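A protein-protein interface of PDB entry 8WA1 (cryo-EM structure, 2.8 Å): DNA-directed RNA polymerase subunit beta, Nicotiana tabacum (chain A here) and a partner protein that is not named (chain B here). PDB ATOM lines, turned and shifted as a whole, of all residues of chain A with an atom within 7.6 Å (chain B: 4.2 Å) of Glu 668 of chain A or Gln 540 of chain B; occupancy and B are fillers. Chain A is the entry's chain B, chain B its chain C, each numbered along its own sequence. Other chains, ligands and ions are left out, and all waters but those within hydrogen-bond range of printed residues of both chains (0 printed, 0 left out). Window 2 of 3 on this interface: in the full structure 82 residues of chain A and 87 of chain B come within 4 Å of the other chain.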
ATOM      1  N   GLY A 664      11.907  26.162   5.044  1.00  0.00           N
ATOM      2  CA  GLY A 664      12.263  26.691   6.334  1.00  0.00           C
ATOM      3  C   GLY A 664      11.316  27.695   6.879  1.00  0.00           C
ATOM      4  O   GLY A 664      11.417  28.087   8.019  1.00  0.00           O
ATOM      5  N   TYR A 665      10.371  28.108   6.072  1.00  0.00           N
ATOM      6  CA  TYR A 665       9.445  29.114   6.505  1.00  0.00           C
ATOM      7  C   TYR A 665       8.466  28.548   7.489  1.00  0.00           C
ATOM      8  O   TYR A 665       7.722  29.284   8.101  1.00  0.00           O
ATOM      9  CB  TYR A 665       8.786  29.766   5.323  1.00  0.00           C
ATOM     10  CG  TYR A 665       9.733  30.656   4.580  1.00  0.00           C
ATOM     11  CD1 TYR A 665       9.997  31.934   5.031  1.00  0.00           C
ATOM     12  CD2 TYR A 665      10.380  30.218   3.442  1.00  0.00           C
ATOM     13  CE1 TYR A 665      10.872  32.756   4.364  1.00  0.00           C
ATOM     14  CE2 TYR A 665      11.258  31.031   2.767  1.00  0.00           C
ATOM     15  CZ  TYR A 665      11.500  32.298   3.236  1.00  0.00           C
ATOM     16  OH  TYR A 665      12.374  33.117   2.569  1.00  0.00           O
ATOM     17  N   ASN A 666       8.435  27.239   7.623  1.00  0.00           N
ATOM     18  CA  ASN A 666       7.569  26.594   8.579  1.00  0.00           C
ATOM     19  C   ASN A 666       8.316  26.088   9.802  1.00  0.00           C
ATOM     20  O   ASN A 666       7.755  25.322  10.560  1.00  0.00           O
ATOM     21  CB  ASN A 666       6.885  25.408   7.925  1.00  0.00           C
ATOM     22  CG  ASN A 666       5.936  25.807   6.841  1.00  0.00           C
ATOM     23  OD1 ASN A 666       5.566  26.968   6.723  1.00  0.00           O
ATOM     24  ND2 ASN A 666       5.523  24.841   6.045  1.00  0.00           N
ATOM     25  N   SER A 667       9.567  26.476  10.017  1.00  0.00           N
ATOM     26  CA  SER A 667      10.338  25.913  11.123  1.00  0.00           C
ATOM     27  C   SER A 667       9.680  26.240  12.407  1.00  0.00           C
ATOM     28  O   SER A 667       9.106  27.302  12.542  1.00  0.00           O
ATOM     29  CB  SER A 667      11.769  26.408  11.155  1.00  0.00           C
ATOM     30  OG  SER A 667      12.559  25.675  12.074  1.00  0.00           O
ATOM     31  N   GLU A 668       9.809  25.359  13.381  1.00  0.00           N
ATOM     32  CA  GLU A 668       9.121  25.533  14.642  1.00  0.00           C
ATOM     33  C   GLU A 668       7.702  25.660  14.246  1.00  0.00           C
ATOM     34  O   GLU A 668       7.210  24.857  13.467  1.00  0.00           O
ATOM     35  CB  GLU A 668       9.600  26.733  15.423  1.00  0.00           C
ATOM     36  CG  GLU A 668      10.683  26.412  16.435  1.00  0.00           C
ATOM     37  CD  GLU A 668      11.963  25.914  15.798  1.00  0.00           C
ATOM     38  OE1 GLU A 668      12.525  24.924  16.305  1.00  0.00           O
ATOM     39  OE2 GLU A 668      12.404  26.505  14.790  1.00  0.00           O
ATOM     40  N   ASP A 669       7.006  26.636  14.767  1.00  0.00           N
ATOM     41  CA  ASP A 669       5.665  26.812  14.295  1.00  0.00           C
ATOM     42  C   ASP A 669       5.660  28.103  13.581  1.00  0.00           C
ATOM     43  O   ASP A 669       5.963  29.112  14.157  1.00  0.00           O
ATOM     44  CB  ASP A 669       4.722  26.901  15.461  1.00  0.00           C
ATOM     45  CG  ASP A 669       4.677  25.631  16.274  1.00  0.00           C
ATOM     46  OD1 ASP A 669       5.068  24.570  15.750  1.00  0.00           O
ATOM     47  OD2 ASP A 669       4.233  25.694  17.438  1.00  0.00           O
ATOM     48  N   ALA A 670       5.302  28.086  12.327  1.00  0.00           N
ATOM     49  CA  ALA A 670       5.292  29.285  11.557  1.00  0.00           C
ATOM     50  C   ALA A 670       4.523  28.913  10.343  1.00  0.00           C
ATOM     51  O   ALA A 670       4.563  27.768   9.935  1.00  0.00           O
ATOM     52  CB  ALA A 670       6.683  29.693  11.204  1.00  0.00           C
ATOM     53  N   VAL A 671       3.810  29.848   9.751  1.00  0.00           N
ATOM     54  CA  VAL A 671       2.949  29.512   8.659  1.00  0.00           C
ATOM     55  C   VAL A 671       3.324  30.322   7.460  1.00  0.00           C
ATOM     56  O   VAL A 671       3.727  31.450   7.596  1.00  0.00           O
ATOM     57  CB  VAL A 671       1.503  29.808   9.039  1.00  0.00           C
ATOM     58  CG1 VAL A 671       0.549  29.126   8.079  1.00  0.00           C
ATOM     59  CG2 VAL A 671       1.213  29.349  10.454  1.00  0.00           C
ATOM     60  N   LYS A 827      -1.139  26.419  16.790  1.00  0.00           N
ATOM     61  CA  LYS A 827      -0.958  27.857  16.789  1.00  0.00           C
ATOM     62  C   LYS A 827       0.284  28.189  16.012  1.00  0.00           C
ATOM     63  O   LYS A 827       1.212  27.408  16.001  1.00  0.00           O
ATOM     64  CB  LYS A 827      -0.792  28.316  18.216  1.00  0.00           C
ATOM     65  CG  LYS A 827      -0.456  29.777  18.411  1.00  0.00           C
ATOM     66  CD  LYS A 827      -0.260  30.066  19.886  1.00  0.00           C
ATOM     67  CE  LYS A 827       0.573  28.986  20.550  1.00  0.00           C
ATOM     68  NZ  LYS A 827       0.809  29.285  21.987  1.00  0.00           N
ATOM     69  N   GLY A 828       0.312  29.328  15.341  1.00  0.00           N
ATOM     70  CA  GLY A 828       1.456  29.710  14.538  1.00  0.00           C
ATOM     71  C   GLY A 828       1.555  31.181  14.256  1.00  0.00           C
ATOM     72  O   GLY A 828       0.601  31.886  14.473  1.00  0.00           O
ATOM     73  N   PHE A 852       1.531  24.281   6.556  1.00  0.00           N
ATOM     74  CA  PHE A 852       1.861  24.058   7.955  1.00  0.00           C
ATOM     75  C   PHE A 852       2.963  23.023   8.133  1.00  0.00           C
ATOM     76  O   PHE A 852       3.218  22.264   7.227  1.00  0.00           O
ATOM     77  CB  PHE A 852       0.630  23.575   8.683  1.00  0.00           C
ATOM     78  CG  PHE A 852      -0.321  24.653   9.088  1.00  0.00           C
ATOM     79  CD1 PHE A 852      -1.248  25.143   8.202  1.00  0.00           C
ATOM     80  CD2 PHE A 852      -0.316  25.140  10.376  1.00  0.00           C
ATOM     81  CE1 PHE A 852      -2.137  26.122   8.580  1.00  0.00           C
ATOM     82  CE2 PHE A 852      -1.201  26.120  10.765  1.00  0.00           C
ATOM     83  CZ  PHE A 852      -2.115  26.612   9.863  1.00  0.00           C
ATOM     84  N   ASN A 853       3.609  22.968   9.290  1.00  0.00           N
ATOM     85  CA  ASN A 853       4.721  22.054   9.516  1.00  0.00           C
ATOM     86  C   ASN A 853       4.187  20.690   9.939  1.00  0.00           C
ATOM     87  O   ASN A 853       3.427  20.609  10.910  1.00  0.00           O
ATOM     88  CB  ASN A 853       5.656  22.610  10.579  1.00  0.00           C
ATOM     89  CG  ASN A 853       6.909  21.775  10.744  1.00  0.00           C
ATOM     90  OD1 ASN A 853       7.045  21.026  11.708  1.00  0.00           O
ATOM     91  ND2 ASN A 853       7.830  21.896   9.796  1.00  0.00           N
ATOM     92  N   PRO A 854       4.549  19.605   9.246  1.00  0.00           N
ATOM     93  CA  PRO A 854       3.989  18.289   9.581  1.00  0.00           C
ATOM     94  C   PRO A 854       4.617  17.633  10.800  1.00  0.00           C
ATOM     95  O   PRO A 854       4.162  16.554  11.197  1.00  0.00           O
ATOM     96  CB  PRO A 854       4.268  17.469   8.317  1.00  0.00           C
ATOM     97  CG  PRO A 854       5.521  18.068   7.778  1.00  0.00           C
ATOM     98  CD  PRO A 854       5.444  19.544   8.078  1.00  0.00           C
ATOM     99  N   LEU A 855       5.634  18.235  11.408  1.00  0.00           N
ATOM    100  CA  LEU A 855       6.289  17.644  12.568  1.00  0.00           C
ATOM    101  C   LEU A 855       5.609  18.010  13.881  1.00  0.00           C
ATOM    102  O   LEU A 855       6.014  17.503  14.932  1.00  0.00           O
ATOM    103  CB  LEU A 855       7.764  18.062  12.622  1.00  0.00           C
ATOM    104  CG  LEU A 855       8.752  17.325  11.714  1.00  0.00           C
ATOM    105  CD1 LEU A 855       8.583  17.717  10.254  1.00  0.00           C
ATOM    106  CD2 LEU A 855      10.173  17.584  12.175  1.00  0.00           C
ATOM    107  N   GLY A 856       4.591  18.870  13.847  1.00  0.00           N
ATOM    108  CA  GLY A 856       3.892  19.214  15.072  1.00  0.00           C
ATOM    109  C   GLY A 856       2.984  18.099  15.558  1.00  0.00           C
ATOM    110  O   GLY A 856       2.736  17.968  16.760  1.00  0.00           O
ATOM    111  N   SER A 859       4.643  15.794  17.948  1.00  0.00           N
ATOM    112  CA  SER A 859       5.120  16.539  19.109  1.00  0.00           C
ATOM    113  C   SER A 859       3.986  16.840  20.084  1.00  0.00           C
ATOM    114  O   SER A 859       4.029  16.412  21.242  1.00  0.00           O
ATOM    115  CB  SER A 859       5.796  17.834  18.662  1.00  0.00           C
ATOM    116  OG  SER A 859       4.851  18.737  18.114  1.00  0.00           O
ATOM    117  N   ALA B 495      13.695  29.503  21.759  1.00  0.00           N
ATOM    118  CA  ALA B 495      12.684  30.263  21.065  1.00  0.00           C
ATOM    119  C   ALA B 495      11.909  29.491  20.051  1.00  0.00           C
ATOM    120  O   ALA B 495      12.474  28.720  19.296  1.00  0.00           O
ATOM    121  CB  ALA B 495      13.327  31.441  20.389  1.00  0.00           C
ATOM    122  N   ASP B 496      10.607  29.697  20.022  1.00  0.00           N
ATOM    123  CA  ASP B 496       9.773  29.069  19.034  1.00  0.00           C
ATOM    124  C   ASP B 496       8.937  30.187  18.535  1.00  0.00           C
ATOM    125  O   ASP B 496       8.687  31.138  19.252  1.00  0.00           O
ATOM    126  CB  ASP B 496       8.906  27.955  19.612  1.00  0.00           C
ATOM    127  CG  ASP B 496       8.286  28.292  20.968  1.00  0.00           C
ATOM    128  OD1 ASP B 496       8.591  29.332  21.583  1.00  0.00           O
ATOM    129  OD2 ASP B 496       7.468  27.478  21.437  1.00  0.00           O
ATOM    130  N   PHE B 497       8.540  30.122  17.286  1.00  0.00           N
ATOM    131  CA  PHE B 497       7.791  31.209  16.716  1.00  0.00           C
ATOM    132  C   PHE B 497       6.302  31.026  16.926  1.00  0.00           C
ATOM    133  O   PHE B 497       5.531  31.064  15.990  1.00  0.00           O
ATOM    134  CB  PHE B 497       8.193  31.342  15.266  1.00  0.00           C
ATOM    135  CG  PHE B 497       9.674  31.298  15.072  1.00  0.00           C
ATOM    136  CD1 PHE B 497      10.446  32.402  15.355  1.00  0.00           C
ATOM    137  CD2 PHE B 497      10.297  30.143  14.659  1.00  0.00           C
ATOM    138  CE1 PHE B 497      11.813  32.369  15.201  1.00  0.00           C
ATOM    139  CE2 PHE B 497      11.665  30.097  14.508  1.00  0.00           C
ATOM    140  CZ  PHE B 497      12.423  31.216  14.774  1.00  0.00           C
ATOM    141  N   THR B 539      17.922  20.727  13.798  1.00  0.00           N
ATOM    142  CA  THR B 539      16.983  20.251  14.806  1.00  0.00           C
ATOM    143  C   THR B 539      15.761  19.546  14.232  1.00  0.00           C
ATOM    144  O   THR B 539      15.569  18.356  14.490  1.00  0.00           O
ATOM    145  CB  THR B 539      16.542  21.423  15.697  1.00  0.00           C
ATOM    146  OG1 THR B 539      15.304  21.101  16.345  1.00  0.00           O
ATOM    147  CG2 THR B 539      16.382  22.703  14.881  1.00  0.00           C
ATOM    148  N   GLN B 540      14.928  20.232  13.448  1.00  0.00           N
ATOM    149  CA  GLN B 540      13.640  19.650  13.082  1.00  0.00           C
ATOM    150  C   GLN B 540      13.515  19.338  11.596  1.00  0.00           C
ATOM    151  O   GLN B 540      13.243  18.193  11.225  1.00  0.00           O
ATOM    152  CB  GLN B 540      12.505  20.582  13.505  1.00  0.00           C
ATOM    153  CG  GLN B 540      12.420  20.800  15.002  1.00  0.00           C
ATOM    154  CD  GLN B 540      11.267  21.697  15.393  1.00  0.00           C
ATOM    155  OE1 GLN B 540      10.463  22.095  14.552  1.00  0.00           O
ATOM    156  NE2 GLN B 540      11.180  22.019  16.677  1.00  0.00           N
ATOM    157  N   ASP B 541      13.705  20.339  10.736  1.00  0.00           N
ATOM    158  CA  ASP B 541      13.497  20.111   9.310  1.00  0.00           C
ATOM    159  C   ASP B 541      14.802  19.786   8.595  1.00  0.00           C
ATOM    160  O   ASP B 541      14.826  18.922   7.710  1.00  0.00           O
ATOM    161  CB  ASP B 541      12.827  21.331   8.677  1.00  0.00           C
ATOM    162  CG  ASP B 541      11.485  21.651   9.308  1.00  0.00           C
ATOM    163  OD1 ASP B 541      11.090  20.945  10.260  1.00  0.00           O
ATOM    164  OD2 ASP B 541      10.825  22.609   8.853  1.00  0.00           O
ATOM    165  N   MET B 542      15.891  20.464   8.963  1.00  0.00           N
ATOM    166  CA  MET B 542      17.191  20.150   8.383  1.00  0.00           C
ATOM    167  C   MET B 542      17.621  18.736   8.749  1.00  0.00           C
ATOM    168  O   MET B 542      18.235  18.030   7.940  1.00  0.00           O
ATOM    169  CB  MET B 542      18.228  21.173   8.845  1.00  0.00           C
ATOM    170  CG  MET B 542      17.682  22.185   9.836  1.00  0.00           C
ATOM    171  SD  MET B 542      18.898  23.418  10.322  1.00  0.00           S
ATOM    172  CE  MET B 542      17.892  24.495  11.337  1.00  0.00           C
ATOM    173  N   ILE B 544      15.535  16.238   9.230  1.00  0.00           N
ATOM    174  CA  ILE B 544      14.734  15.367   8.373  1.00  0.00           C
ATOM    175  C   ILE B 544      15.330  15.304   6.972  1.00  0.00           C
ATOM    176  O   ILE B 544      15.433  14.226   6.373  1.00  0.00           O
ATOM    177  CB  ILE B 544      13.269  15.843   8.346  1.00  0.00           C
ATOM    178  CG1 ILE B 544      12.583  15.530   9.676  1.00  0.00           C
ATOM    179  CG2 ILE B 544      12.512  15.199   7.196  1.00  0.00           C
ATOM    180  CD1 ILE B 544      12.567  14.060  10.022  1.00  0.00           C
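OE1 of Glu 668 of chain A is in hydrogen-bond range of NE2 of Gln 540 of chain B, 3.2 Å away. The backbone carbonyl oxygen (O) of Asp 669 of chain A lies close to the backbone carbonyl oxygen (O) of Phe 497 of chain B, at 2.7 Å. The side-chain amide nitrogen (ND2) of Asn 853 of chain A sits at hydrogen-bond distance from the side-chain carboxylate (OD2) of Asp 541 of chain B (3.2 Å).
The side-chain hydroxyl (OG) of Ser 667 of chain A sits at hydrogen-bond distance from the side-chain carboxylate (OE2) of Glu 668 of chain A (2.8 Å). N of Leu 855 of chain A sits at hydrogen-bond distance from OD1 of Asn 853 of chain A.
Among the printed residues, merely in contact across the chains: Ser 667 of chain A with Phe 497 of chain B, Glu 668 of chain A with Asp 496 of chain B, Glu 668 of chain A with Phe 497 of chain B, Leu 855 of chain A with Gln 540 of chain B and Leu 855 of chain A with Asp 541 of chain B.
Glu 668 of chain A touches three residues of chain B. Gln 540 of chain B touches just these residues of chain A: Glu 668 (3.2 Å) and Leu 855 (3.3 Å). No residue of chain A comes within 4 Å of Thr 539 of chain B. Printed residues of chain B within 4 Å of Ser 667 of chain A: Phe 497 (3.7 Å). Of the printed residues of chain B, Asn 853 of chain A touches Asp 541 (3.2 Å). Printed residues of chain A within 4 Å of Phe 497 of chain B: Ser 667, Glu 668 and Asp 669. Of the printed residues of chain B, Asp 669 of chain A touches Phe 497 (2.7 Å). Of the printed residues of chain A, Asp 496 of chain B touches Glu 668 (3.8 Å). Ser 859 of chain A touches none of the printed residues of chain B. The nearest residue of chain A that does not touch Gln 540 of chain B is Asn 853 of chain A (4.6 Å). The nearest printed residue of chain A that does not touch Asp 541 of chain B is Ser 667 of chain A (4.04 Å).
Printed residues of chain A that touch a printed residue of chain B: Ser 667, Glu 668, Asp 669, Asn 853 and Leu 855. Of the 8 printed residues of chain B, 4 touch a printed residue of chain A. Among the printed residues, no Asp or Glu carboxylate lies within 4 Å of a Lys or Arg side-chain nitrogen of the other chain.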
